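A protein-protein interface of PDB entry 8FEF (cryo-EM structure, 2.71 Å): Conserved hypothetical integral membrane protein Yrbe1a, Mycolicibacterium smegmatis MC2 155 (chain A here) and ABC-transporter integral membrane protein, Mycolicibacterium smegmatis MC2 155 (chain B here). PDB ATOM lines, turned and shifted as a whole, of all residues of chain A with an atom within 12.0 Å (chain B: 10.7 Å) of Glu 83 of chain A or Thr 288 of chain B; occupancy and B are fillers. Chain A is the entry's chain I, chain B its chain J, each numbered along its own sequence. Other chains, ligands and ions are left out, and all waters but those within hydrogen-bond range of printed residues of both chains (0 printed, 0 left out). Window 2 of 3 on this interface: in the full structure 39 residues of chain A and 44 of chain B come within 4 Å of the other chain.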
ATOM      1  N   ILE A  74       0.918 -34.352   4.201  1.00  0.00           N
ATOM      2  CA  ILE A  74      -0.531 -34.225   4.084  1.00  0.00           C
ATOM      3  C   ILE A  74      -0.982 -32.821   4.463  1.00  0.00           C
ATOM      4  O   ILE A  74      -1.860 -32.247   3.813  1.00  0.00           O
ATOM      5  CB  ILE A  74      -1.232 -35.304   4.928  1.00  0.00           C
ATOM      6  CG1 ILE A  74      -0.946 -36.683   4.340  1.00  0.00           C
ATOM      7  CG2 ILE A  74      -2.729 -35.063   4.993  1.00  0.00           C
ATOM      8  CD1 ILE A  74      -1.168 -36.762   2.863  1.00  0.00           C
ATOM      9  N   PHE A  75      -0.396 -32.248   5.517  1.00  0.00           N
ATOM     10  CA  PHE A  75      -0.752 -30.891   5.923  1.00  0.00           C
ATOM     11  C   PHE A  75      -0.442 -29.888   4.818  1.00  0.00           C
ATOM     12  O   PHE A  75      -1.281 -29.040   4.479  1.00  0.00           O
ATOM     13  CB  PHE A  75      -0.011 -30.533   7.213  1.00  0.00           C
ATOM     14  CG  PHE A  75      -0.042 -29.070   7.550  1.00  0.00           C
ATOM     15  CD1 PHE A  75      -1.138 -28.514   8.183  1.00  0.00           C
ATOM     16  CD2 PHE A  75       1.041 -28.254   7.259  1.00  0.00           C
ATOM     17  CE1 PHE A  75      -1.164 -27.172   8.498  1.00  0.00           C
ATOM     18  CE2 PHE A  75       1.019 -26.912   7.572  1.00  0.00           C
ATOM     19  CZ  PHE A  75      -0.084 -26.371   8.194  1.00  0.00           C
ATOM     20  N   THR A  76       0.761 -29.975   4.241  1.00  0.00           N
ATOM     21  CA  THR A  76       1.135 -29.057   3.167  1.00  0.00           C
ATOM     22  C   THR A  76       0.206 -29.209   1.969  1.00  0.00           C
ATOM     23  O   THR A  76      -0.295 -28.217   1.422  1.00  0.00           O
ATOM     24  CB  THR A  76       2.587 -29.298   2.754  1.00  0.00           C
ATOM     25  OG1 THR A  76       3.455 -28.988   3.851  1.00  0.00           O
ATOM     26  CG2 THR A  76       2.958 -28.434   1.562  1.00  0.00           C
ATOM     27  N   LEU A  77      -0.049 -30.455   1.559  1.00  0.00           N
ATOM     28  CA  LEU A  77      -0.914 -30.700   0.412  1.00  0.00           C
ATOM     29  C   LEU A  77      -2.321 -30.174   0.661  1.00  0.00           C
ATOM     30  O   LEU A  77      -2.916 -29.533  -0.213  1.00  0.00           O
ATOM     31  CB  LEU A  77      -0.944 -32.195   0.098  1.00  0.00           C
ATOM     32  CG  LEU A  77      -1.649 -32.639  -1.181  1.00  0.00           C
ATOM     33  CD1 LEU A  77      -0.891 -32.157  -2.406  1.00  0.00           C
ATOM     34  CD2 LEU A  77      -1.789 -34.145  -1.194  1.00  0.00           C
ATOM     35  N   ASN A  78      -2.860 -30.416   1.859  1.00  0.00           N
ATOM     36  CA  ASN A  78      -4.220 -29.991   2.165  1.00  0.00           C
ATOM     37  C   ASN A  78      -4.346 -28.476   2.182  1.00  0.00           C
ATOM     38  O   ASN A  78      -5.315 -27.936   1.643  1.00  0.00           O
ATOM     39  CB  ASN A  78      -4.671 -30.574   3.502  1.00  0.00           C
ATOM     40  CG  ASN A  78      -5.062 -32.031   3.400  1.00  0.00           C
ATOM     41  OD1 ASN A  78      -5.265 -32.552   2.308  1.00  0.00           O
ATOM     42  ND2 ASN A  78      -5.180 -32.693   4.543  1.00  0.00           N
ATOM     43  N   ILE A  79      -3.390 -27.767   2.791  1.00  0.00           N
ATOM     44  CA  ILE A  79      -3.516 -26.310   2.830  1.00  0.00           C
ATOM     45  C   ILE A  79      -3.359 -25.718   1.431  1.00  0.00           C
ATOM     46  O   ILE A  79      -4.118 -24.817   1.036  1.00  0.00           O
ATOM     47  CB  ILE A  79      -2.539 -25.683   3.848  1.00  0.00           C
ATOM     48  CG1 ILE A  79      -1.076 -25.949   3.495  1.00  0.00           C
ATOM     49  CG2 ILE A  79      -2.842 -26.178   5.253  1.00  0.00           C
ATOM     50  CD1 ILE A  79      -0.099 -25.221   4.381  1.00  0.00           C
ATOM     51  N   LEU A  80      -2.393 -26.219   0.650  1.00  0.00           N
ATOM     52  CA  LEU A  80      -2.200 -25.692  -0.697  1.00  0.00           C
ATOM     53  C   LEU A  80      -3.413 -25.957  -1.579  1.00  0.00           C
ATOM     54  O   LEU A  80      -3.812 -25.094  -2.368  1.00  0.00           O
ATOM     55  CB  LEU A  80      -0.935 -26.280  -1.322  1.00  0.00           C
ATOM     56  CG  LEU A  80       0.388 -25.879  -0.661  1.00  0.00           C
ATOM     57  CD1 LEU A  80       1.568 -26.442  -1.434  1.00  0.00           C
ATOM     58  CD2 LEU A  80       0.500 -24.369  -0.526  1.00  0.00           C
ATOM     59  N   LEU A  81      -4.025 -27.138  -1.455  1.00  0.00           N
ATOM     60  CA  LEU A  81      -5.200 -27.446  -2.267  1.00  0.00           C
ATOM     61  C   LEU A  81      -6.435 -26.691  -1.789  1.00  0.00           C
ATOM     62  O   LEU A  81      -7.278 -26.302  -2.606  1.00  0.00           O
ATOM     63  CB  LEU A  81      -5.452 -28.952  -2.277  1.00  0.00           C
ATOM     64  CG  LEU A  81      -4.459 -29.736  -3.134  1.00  0.00           C
ATOM     65  CD1 LEU A  81      -4.806 -31.202  -3.140  1.00  0.00           C
ATOM     66  CD2 LEU A  81      -4.425 -29.189  -4.551  1.00  0.00           C
ATOM     67  N   ALA A  82      -6.575 -26.490  -0.477  1.00  0.00           N
ATOM     68  CA  ALA A  82      -7.698 -25.716   0.037  1.00  0.00           C
ATOM     69  C   ALA A  82      -7.643 -24.277  -0.454  1.00  0.00           C
ATOM     70  O   ALA A  82      -8.675 -23.695  -0.803  1.00  0.00           O
ATOM     71  CB  ALA A  82      -7.717 -25.765   1.565  1.00  0.00           C
ATOM     72  N   GLU A  83      -6.448 -23.681  -0.479  1.00  0.00           N
ATOM     73  CA  GLU A  83      -6.318 -22.375  -1.122  1.00  0.00           C
ATOM     74  C   GLU A  83      -6.561 -22.472  -2.623  1.00  0.00           C
ATOM     75  O   GLU A  83      -7.163 -21.573  -3.220  1.00  0.00           O
ATOM     76  CB  GLU A  83      -4.946 -21.777  -0.833  1.00  0.00           C
ATOM     77  CG  GLU A  83      -4.776 -21.360   0.607  1.00  0.00           C
ATOM     78  CD  GLU A  83      -5.808 -20.335   1.045  1.00  0.00           C
ATOM     79  OE1 GLU A  83      -6.114 -19.418   0.254  1.00  0.00           O
ATOM     80  OE2 GLU A  83      -6.320 -20.450   2.178  1.00  0.00           O
ATOM     81  N   PHE A  84      -6.091 -23.554  -3.251  1.00  0.00           N
ATOM     82  CA  PHE A  84      -6.358 -23.788  -4.665  1.00  0.00           C
ATOM     83  C   PHE A  84      -7.851 -23.931  -4.932  1.00  0.00           C
ATOM     84  O   PHE A  84      -8.339 -23.505  -5.985  1.00  0.00           O
ATOM     85  CB  PHE A  84      -5.610 -25.045  -5.117  1.00  0.00           C
ATOM     86  CG  PHE A  84      -5.294 -25.085  -6.586  1.00  0.00           C
ATOM     87  CD1 PHE A  84      -6.287 -25.313  -7.522  1.00  0.00           C
ATOM     88  CD2 PHE A  84      -3.989 -24.926  -7.026  1.00  0.00           C
ATOM     89  CE1 PHE A  84      -5.991 -25.360  -8.869  1.00  0.00           C
ATOM     90  CE2 PHE A  84      -3.685 -24.975  -8.372  1.00  0.00           C
ATOM     91  CZ  PHE A  84      -4.688 -25.191  -9.295  1.00  0.00           C
ATOM     92  N   GLY A  85      -8.591 -24.516  -3.990  1.00  0.00           N
ATOM     93  CA  GLY A  85     -10.009 -24.771  -4.133  1.00  0.00           C
ATOM     94  C   GLY A  85     -10.362 -26.229  -4.334  1.00  0.00           C
ATOM     95  O   GLY A  85     -11.509 -26.615  -4.075  1.00  0.00           O
ATOM     96  N   ALA A  86      -9.411 -27.050  -4.785  1.00  0.00           N
ATOM     97  CA  ALA A  86      -9.653 -28.467  -5.052  1.00  0.00           C
ATOM     98  C   ALA A  86      -9.136 -29.303  -3.883  1.00  0.00           C
ATOM     99  O   ALA A  86      -8.100 -29.957  -3.959  1.00  0.00           O
ATOM    100  CB  ALA A  86      -8.999 -28.878  -6.367  1.00  0.00           C
ATOM    101  N   ALA A  87      -9.891 -29.285  -2.789  1.00  0.00           N
ATOM    102  CA  ALA A  87      -9.516 -30.016  -1.587  1.00  0.00           C
ATOM    103  C   ALA A  87     -10.062 -31.437  -1.555  1.00  0.00           C
ATOM    104  O   ALA A  87      -9.765 -32.178  -0.612  1.00  0.00           O
ATOM    105  CB  ALA A  87      -9.985 -29.258  -0.341  1.00  0.00           C
ATOM    106  N   ASP A  88     -10.854 -31.834  -2.550  1.00  0.00           N
ATOM    107  CA  ASP A  88     -11.405 -33.182  -2.614  1.00  0.00           C
ATOM    108  C   ASP A  88     -10.484 -34.173  -3.308  1.00  0.00           C
ATOM    109  O   ASP A  88     -10.703 -35.383  -3.193  1.00  0.00           O
ATOM    110  CB  ASP A  88     -12.759 -33.166  -3.330  1.00  0.00           C
ATOM    111  CG  ASP A  88     -13.818 -32.414  -2.554  1.00  0.00           C
ATOM    112  OD1 ASP A  88     -13.732 -32.384  -1.309  1.00  0.00           O
ATOM    113  OD2 ASP A  88     -14.735 -31.853  -3.189  1.00  0.00           O
ATOM    114  N   VAL A  89      -9.463 -33.695  -4.017  1.00  0.00           N
ATOM    115  CA  VAL A  89      -8.527 -34.558  -4.728  1.00  0.00           C
ATOM    116  C   VAL A  89      -7.247 -34.779  -3.933  1.00  0.00           C
ATOM    117  O   VAL A  89      -6.315 -35.425  -4.428  1.00  0.00           O
ATOM    118  CB  VAL A  89      -8.215 -33.996  -6.121  1.00  0.00           C
ATOM    119  CG1 VAL A  89      -9.463 -34.018  -6.984  1.00  0.00           C
ATOM    120  CG2 VAL A  89      -7.677 -32.582  -6.003  1.00  0.00           C
ATOM    121  N   SER A  90      -7.194 -34.278  -2.695  1.00  0.00           N
ATOM    122  CA  SER A  90      -5.989 -34.368  -1.876  1.00  0.00           C
ATOM    123  C   SER A  90      -5.539 -35.810  -1.708  1.00  0.00           C
ATOM    124  O   SER A  90      -4.345 -36.114  -1.840  1.00  0.00           O
ATOM    125  CB  SER A  90      -6.236 -33.722  -0.514  1.00  0.00           C
ATOM    126  OG  SER A  90      -7.275 -34.388   0.181  1.00  0.00           O
ATOM    127  N   GLN A 181      -7.847 -31.127   9.727  1.00  0.00           N
ATOM    128  CA  GLN A 181      -8.061 -30.135   8.684  1.00  0.00           C
ATOM    129  C   GLN A 181      -9.463 -30.195   8.096  1.00  0.00           C
ATOM    130  O   GLN A 181      -9.757 -29.449   7.157  1.00  0.00           O
ATOM    131  CB  GLN A 181      -7.015 -30.307   7.582  1.00  0.00           C
ATOM    132  CG  GLN A 181      -5.597 -30.131   8.082  1.00  0.00           C
ATOM    133  CD  GLN A 181      -4.576 -30.194   6.974  1.00  0.00           C
ATOM    134  OE1 GLN A 181      -4.141 -31.275   6.580  1.00  0.00           O
ATOM    135  NE2 GLN A 181      -4.186 -29.035   6.461  1.00  0.00           N
ATOM    136  N   ASN A 182     -10.319 -31.071   8.629  1.00  0.00           N
ATOM    137  CA  ASN A 182     -11.748 -31.120   8.310  1.00  0.00           C
ATOM    138  C   ASN A 182     -12.004 -31.318   6.818  1.00  0.00           C
ATOM    139  O   ASN A 182     -12.907 -30.708   6.242  1.00  0.00           O
ATOM    140  CB  ASN A 182     -12.466 -29.869   8.817  1.00  0.00           C
ATOM    141  CG  ASN A 182     -12.461 -29.767  10.326  1.00  0.00           C
ATOM    142  OD1 ASN A 182     -12.511 -30.777  11.028  1.00  0.00           O
ATOM    143  ND2 ASN A 182     -12.398 -28.542  10.837  1.00  0.00           N
ATOM    144  N   VAL A 183     -11.209 -32.173   6.180  1.00  0.00           N
ATOM    145  CA  VAL A 183     -11.520 -32.589   4.818  1.00  0.00           C
ATOM    146  C   VAL A 183     -12.526 -33.729   4.896  1.00  0.00           C
ATOM    147  O   VAL A 183     -12.752 -34.298   5.969  1.00  0.00           O
ATOM    148  CB  VAL A 183     -10.259 -33.006   4.039  1.00  0.00           C
ATOM    149  CG1 VAL A 183      -9.190 -31.933   4.143  1.00  0.00           C
ATOM    150  CG2 VAL A 183      -9.738 -34.341   4.535  1.00  0.00           C
ATOM    151  N   PHE B 108       1.961 -25.371 -14.179  1.00  0.00           N
ATOM    152  CA  PHE B 108       2.088 -25.090 -12.758  1.00  0.00           C
ATOM    153  C   PHE B 108       3.291 -25.771 -12.121  1.00  0.00           C
ATOM    154  O   PHE B 108       3.467 -25.658 -10.902  1.00  0.00           O
ATOM    155  CB  PHE B 108       0.817 -25.518 -12.018  1.00  0.00           C
ATOM    156  CG  PHE B 108      -0.379 -24.660 -12.313  1.00  0.00           C
ATOM    157  CD1 PHE B 108      -0.228 -23.372 -12.792  1.00  0.00           C
ATOM    158  CD2 PHE B 108      -1.659 -25.142 -12.096  1.00  0.00           C
ATOM    159  CE1 PHE B 108      -1.329 -22.583 -13.055  1.00  0.00           C
ATOM    160  CE2 PHE B 108      -2.763 -24.357 -12.358  1.00  0.00           C
ATOM    161  CZ  PHE B 108      -2.596 -23.077 -12.838  1.00  0.00           C
ATOM    162  N   PHE B 111       5.413 -23.627 -10.099  1.00  0.00           N
ATOM    163  CA  PHE B 111       4.713 -23.327  -8.858  1.00  0.00           C
ATOM    164  C   PHE B 111       4.715 -24.531  -7.924  1.00  0.00           C
ATOM    165  O   PHE B 111       4.833 -24.377  -6.704  1.00  0.00           O
ATOM    166  CB  PHE B 111       3.286 -22.870  -9.171  1.00  0.00           C
ATOM    167  CG  PHE B 111       2.244 -23.437  -8.250  1.00  0.00           C
ATOM    168  CD1 PHE B 111       2.049 -22.912  -6.985  1.00  0.00           C
ATOM    169  CD2 PHE B 111       1.449 -24.494  -8.659  1.00  0.00           C
ATOM    170  CE1 PHE B 111       1.095 -23.444  -6.146  1.00  0.00           C
ATOM    171  CE2 PHE B 111       0.491 -25.025  -7.822  1.00  0.00           C
ATOM    172  CZ  PHE B 111       0.313 -24.497  -6.565  1.00  0.00           C
ATOM    173  N   LEU B 115       7.163 -24.804  -3.886  1.00  0.00           N
ATOM    174  CA  LEU B 115       6.483 -25.150  -2.646  1.00  0.00           C
ATOM    175  C   LEU B 115       6.820 -26.561  -2.197  1.00  0.00           C
ATOM    176  O   LEU B 115       6.710 -26.865  -1.006  1.00  0.00           O
ATOM    177  CB  LEU B 115       4.972 -24.984  -2.810  1.00  0.00           C
ATOM    178  CG  LEU B 115       4.505 -23.536  -2.969  1.00  0.00           C
ATOM    179  CD1 LEU B 115       3.006 -23.474  -3.159  1.00  0.00           C
ATOM    180  CD2 LEU B 115       4.926 -22.707  -1.768  1.00  0.00           C
ATOM    181  N   ARG B 119       8.883 -26.142   1.528  1.00  0.00           N
ATOM    182  CA  ARG B 119       8.039 -26.546   2.648  1.00  0.00           C
ATOM    183  C   ARG B 119       8.485 -27.868   3.263  1.00  0.00           C
ATOM    184  O   ARG B 119       8.575 -27.984   4.490  1.00  0.00           O
ATOM    185  CB  ARG B 119       6.578 -26.632   2.203  1.00  0.00           C
ATOM    186  CG  ARG B 119       6.003 -25.331   1.673  1.00  0.00           C
ATOM    187  CD  ARG B 119       5.924 -24.263   2.745  1.00  0.00           C
ATOM    188  NE  ARG B 119       5.256 -23.065   2.253  1.00  0.00           N
ATOM    189  CZ  ARG B 119       3.954 -22.839   2.356  1.00  0.00           C
ATOM    190  NH1 ARG B 119       3.145 -23.706   2.942  1.00  0.00           N
ATOM    191  NH2 ARG B 119       3.449 -21.714   1.858  1.00  0.00           N
ATOM    192  N   PHE B 214       4.877 -17.382  -7.175  1.00  0.00           N
ATOM    193  CA  PHE B 214       4.279 -18.111  -6.066  1.00  0.00           C
ATOM    194  C   PHE B 214       5.293 -18.516  -5.003  1.00  0.00           C
ATOM    195  O   PHE B 214       4.974 -19.344  -4.143  1.00  0.00           O
ATOM    196  CB  PHE B 214       3.539 -19.342  -6.590  1.00  0.00           C
ATOM    197  CG  PHE B 214       2.387 -19.011  -7.495  1.00  0.00           C
ATOM    198  CD1 PHE B 214       2.577 -18.876  -8.858  1.00  0.00           C
ATOM    199  CD2 PHE B 214       1.117 -18.828  -6.981  1.00  0.00           C
ATOM    200  CE1 PHE B 214       1.521 -18.566  -9.690  1.00  0.00           C
ATOM    201  CE2 PHE B 214       0.058 -18.518  -7.808  1.00  0.00           C
ATOM    202  CZ  PHE B 214       0.261 -18.389  -9.163  1.00  0.00           C
ATOM    203  N   ARG B 216       7.522 -17.087  -1.850  1.00  0.00           N
ATOM    204  CA  ARG B 216       7.677 -15.991  -0.906  1.00  0.00           C
ATOM    205  C   ARG B 216       9.008 -16.134  -0.183  1.00  0.00           C
ATOM    206  O   ARG B 216       9.345 -17.223   0.296  1.00  0.00           O
ATOM    207  CB  ARG B 216       6.527 -15.959   0.103  1.00  0.00           C
ATOM    208  CG  ARG B 216       5.252 -15.316  -0.420  1.00  0.00           C
ATOM    209  CD  ARG B 216       4.308 -16.341  -1.022  1.00  0.00           C
ATOM    210  NE  ARG B 216       3.115 -15.725  -1.591  1.00  0.00           N
ATOM    211  CZ  ARG B 216       2.047 -15.367  -0.890  1.00  0.00           C
ATOM    212  NH1 ARG B 216       1.994 -15.531   0.421  1.00  0.00           N
ATOM    213  NH2 ARG B 216       1.006 -14.832  -1.520  1.00  0.00           N
ATOM    214  N   TYR B 279       2.284 -22.187   9.446  1.00  0.00           N
ATOM    215  CA  TYR B 279       1.185 -22.113   8.492  1.00  0.00           C
ATOM    216  C   TYR B 279      -0.103 -22.723   9.032  1.00  0.00           C
ATOM    217  O   TYR B 279      -0.973 -23.114   8.247  1.00  0.00           O
ATOM    218  CB  TYR B 279       1.577 -22.791   7.179  1.00  0.00           C
ATOM    219  CG  TYR B 279       2.946 -22.396   6.680  1.00  0.00           C
ATOM    220  CD1 TYR B 279       3.141 -21.195   6.016  1.00  0.00           C
ATOM    221  CD2 TYR B 279       4.040 -23.224   6.871  1.00  0.00           C
ATOM    222  CE1 TYR B 279       4.390 -20.828   5.559  1.00  0.00           C
ATOM    223  CE2 TYR B 279       5.292 -22.867   6.418  1.00  0.00           C
ATOM    224  CZ  TYR B 279       5.461 -21.668   5.761  1.00  0.00           C
ATOM    225  OH  TYR B 279       6.707 -21.307   5.307  1.00  0.00           O
ATOM    226  N   GLY B 280      -0.240 -22.819  10.354  1.00  0.00           N
ATOM    227  CA  GLY B 280      -1.449 -23.391  10.925  1.00  0.00           C
ATOM    228  C   GLY B 280      -2.691 -22.579  10.614  1.00  0.00           C
ATOM    229  O   GLY B 280      -3.750 -23.136  10.314  1.00  0.00           O
ATOM    230  N   THR B 281      -2.579 -21.253  10.681  1.00  0.00           N
ATOM    231  CA  THR B 281      -3.697 -20.357  10.415  1.00  0.00           C
ATOM    232  C   THR B 281      -3.607 -19.705   9.040  1.00  0.00           C
ATOM    233  O   THR B 281      -4.572 -19.747   8.271  1.00  0.00           O
ATOM    234  CB  THR B 281      -3.775 -19.276  11.501  1.00  0.00           C
ATOM    235  OG1 THR B 281      -4.037 -19.890  12.769  1.00  0.00           O
ATOM    236  CG2 THR B 281      -4.878 -18.279  11.189  1.00  0.00           C
ATOM    237  N   ASP B 282      -2.462 -19.109   8.710  1.00  0.00           N
ATOM    238  CA  ASP B 282      -2.289 -18.450   7.425  1.00  0.00           C
ATOM    239  C   ASP B 282      -1.431 -19.324   6.525  1.00  0.00           C
ATOM    240  O   ASP B 282      -0.224 -19.456   6.776  1.00  0.00           O
ATOM    241  CB  ASP B 282      -1.644 -17.077   7.606  1.00  0.00           C
ATOM    242  CG  ASP B 282      -1.638 -16.262   6.329  1.00  0.00           C
ATOM    243  OD1 ASP B 282      -2.362 -16.631   5.380  1.00  0.00           O
ATOM    244  OD2 ASP B 282      -0.907 -15.251   6.272  1.00  0.00           O
ATOM    245  N   PRO B 283      -1.995 -19.936   5.481  1.00  0.00           N
ATOM    246  CA  PRO B 283      -1.186 -20.797   4.601  1.00  0.00           C
ATOM    247  C   PRO B 283      -0.129 -20.054   3.803  1.00  0.00           C
ATOM    248  O   PRO B 283       0.772 -20.707   3.264  1.00  0.00           O
ATOM    249  CB  PRO B 283      -2.234 -21.432   3.677  1.00  0.00           C
ATOM    250  CG  PRO B 283      -3.375 -20.478   3.705  1.00  0.00           C
ATOM    251  CD  PRO B 283      -3.410 -19.908   5.083  1.00  0.00           C
ATOM    252  N   ASN B 284      -0.224 -18.725   3.700  1.00  0.00           N
ATOM    253  CA  ASN B 284       0.752 -17.896   2.989  1.00  0.00           C
ATOM    254  C   ASN B 284       0.857 -18.297   1.516  1.00  0.00           C
ATOM    255  O   ASN B 284       1.947 -18.493   0.974  1.00  0.00           O
ATOM    256  CB  ASN B 284       2.120 -17.945   3.679  1.00  0.00           C
ATOM    257  CG  ASN B 284       3.030 -16.808   3.261  1.00  0.00           C
ATOM    258  OD1 ASN B 284       2.570 -15.709   2.955  1.00  0.00           O
ATOM    259  ND2 ASN B 284       4.331 -17.067   3.248  1.00  0.00           N
ATOM    260  N   PHE B 285      -0.300 -18.414   0.865  1.00  0.00           N
ATOM    261  CA  PHE B 285      -0.363 -18.770  -0.548  1.00  0.00           C
ATOM    262  C   PHE B 285      -1.745 -18.422  -1.078  1.00  0.00           C
ATOM    263  O   PHE B 285      -2.753 -18.847  -0.505  1.00  0.00           O
ATOM    264  CB  PHE B 285      -0.065 -20.261  -0.759  1.00  0.00           C
ATOM    265  CG  PHE B 285      -0.530 -20.792  -2.082  1.00  0.00           C
ATOM    266  CD1 PHE B 285       0.092 -20.406  -3.255  1.00  0.00           C
ATOM    267  CD2 PHE B 285      -1.588 -21.682  -2.152  1.00  0.00           C
ATOM    268  CE1 PHE B 285      -0.336 -20.891  -4.472  1.00  0.00           C
ATOM    269  CE2 PHE B 285      -2.020 -22.171  -3.367  1.00  0.00           C
ATOM    270  CZ  PHE B 285      -1.395 -21.776  -4.528  1.00  0.00           C
ATOM    271  N   ASN B 286      -1.790 -17.653  -2.166  1.00  0.00           N
ATOM    272  CA  ASN B 286      -3.040 -17.212  -2.771  1.00  0.00           C
ATOM    273  C   ASN B 286      -3.019 -17.500  -4.264  1.00  0.00           C
ATOM    274  O   ASN B 286      -2.061 -17.139  -4.954  1.00  0.00           O
ATOM    275  CB  ASN B 286      -3.274 -15.715  -2.542  1.00  0.00           C
ATOM    276  CG  ASN B 286      -3.405 -15.361  -1.079  1.00  0.00           C
ATOM    277  OD1 ASN B 286      -2.412 -15.115  -0.396  1.00  0.00           O
ATOM    278  ND2 ASN B 286      -4.637 -15.326  -0.588  1.00  0.00           N
ATOM    279  N   LEU B 287      -4.065 -18.161  -4.757  1.00  0.00           N
ATOM    280  CA  LEU B 287      -4.282 -18.317  -6.189  1.00  0.00           C
ATOM    281  C   LEU B 287      -5.624 -17.763  -6.642  1.00  0.00           C
ATOM    282  O   LEU B 287      -5.683 -17.012  -7.622  1.00  0.00           O
ATOM    283  CB  LEU B 287      -4.168 -19.795  -6.588  1.00  0.00           C
ATOM    284  CG  LEU B 287      -4.393 -20.081  -8.072  1.00  0.00           C
ATOM    285  CD1 LEU B 287      -3.239 -19.554  -8.905  1.00  0.00           C
ATOM    286  CD2 LEU B 287      -4.583 -21.562  -8.297  1.00  0.00           C
ATOM    287  N   THR B 288      -6.706 -18.113  -5.952  1.00  0.00           N
ATOM    288  CA  THR B 288      -8.054 -17.750  -6.359  1.00  0.00           C
ATOM    289  C   THR B 288      -8.402 -16.364  -5.814  1.00  0.00           C
ATOM    290  O   THR B 288      -7.567 -15.680  -5.218  1.00  0.00           O
ATOM    291  CB  THR B 288      -9.051 -18.810  -5.894  1.00  0.00           C
ATOM    292  OG1 THR B 288     -10.371 -18.448  -6.317  1.00  0.00           O
ATOM    293  CG2 THR B 288      -9.030 -18.930  -4.381  1.00  0.00           C
ATOM    294  N   VAL B 289      -9.645 -15.937  -6.013  1.00  0.00           N
ATOM    295  CA  VAL B 289     -10.067 -14.620  -5.556  1.00  0.00           C
ATOM    296  C   VAL B 289     -10.306 -14.651  -4.051  1.00  0.00           C
ATOM    297  O   VAL B 289     -10.515 -13.616  -3.419  1.00  0.00           O
ATOM    298  CB  VAL B 289     -11.337 -14.133  -6.291  1.00  0.00           C
ATOM    299  CG1 VAL B 289     -11.073 -13.955  -7.776  1.00  0.00           C
ATOM    300  CG2 VAL B 289     -12.491 -15.059  -6.048  1.00  0.00           C
ATOM    301  OXT VAL B 289     -10.301 -15.712  -3.428  1.00  0.00           O
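Printed residues of chain B within 4 Å of Phe 75 of chain A: Tyr 279 (3.4 Å).
Thr 76 of chain A touches none of the printed residues of chain B.
Printed residues of chain B within 4 Å of Ile 79 of chain A: Arg 119 (3.9 Å).
Of the printed residues of chain B, Leu 80 of chain A touches Leu 115 (3.7 Å) and Phe 285 (3.6 Å).
No residue of chain B comes within 4 Å of Ala 82 of chain A.
Printed residues of chain B within 4 Å of Phe 84 of chain A: Phe 108 and Leu 287.
No residue of chain B comes within 4 Å of Gly 85 of chain A.
Ser 90 of chain A touches none of the printed residues of chain B.
Of the printed residues of chain A, Leu 115 of chain B touches Leu 80.
Of the printed residues of chain A, Pro 283 of chain B touches Glu 83 (3.3 Å).
No residue of chain A comes within 4 Å of Asn 286 of chain B.
Leu 287 of chain B touches just one residue of chain A: Phe 84.
Printed residues of chain A within 4 Å of Thr 288 of chain B: Glu 83.
The nearest residue of chain A that does not touch Thr 288 of chain B is Phe 84 of chain A (4.7 Å).
The nearest printed residue of chain A that does not touch Phe 108 of chain B is Leu 81 of chain A (9.0 Å).
The side-chain carboxylate (OE1) of Glu 83 of chain A lies close to the backbone carbonyl oxygen (O) of Phe 285 of chain B (3.5 Å).
Printed residues of chain B that touch a printed residue of chain A: Phe 108, Leu 115, Arg 119, Tyr 279, Pro 283, Phe 285, Leu 287 and Thr 288.
Hydrophobic or aromatic side chains of chain B within 4 Å of the printed part of chain A: Phe 108, Leu 115, Pro 283, Phe 285 and Leu 287.
Of the 20 printed residues of chain A, 5 touch a printed residue of chain B.
Printed residues of chain A that touch a printed residue of chain B: Phe 75, Ile 79, Leu 80, Glu 83 and Phe 84.
Hydrophobic or aromatic side chains of chain A within 4 Å of the printed part of chain B: Phe 75, Ile 79, Leu 80 and Phe 84.
Among the printed residues, pairs that only touch across the chains: Glu 83 of chain A with Pro 283 of chain B (3.3 Å), Phe 75 of chain A with Tyr 279 of chain B (3.4 Å), Glu 83 of chain A with Thr 288 of chain B (3.4 Å), Phe 84 of chain A with Leu 287 of chain B (3.5 Å), Leu 80 of chain A with Phe 285 of chain B (3.6 Å), Phe 84 of chain A with Phe 108 of chain B (3.7 Å), Leu 80 of chain A with Leu 115 of chain B (3.7 Å) and Ile 79 of chain A with Arg 119 of chain B (3.9 Å).
NH2 of Arg 119 of chain B sits at hydrogen-bond distance from O of Pro 283 of chain B, 3.2 Å away.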
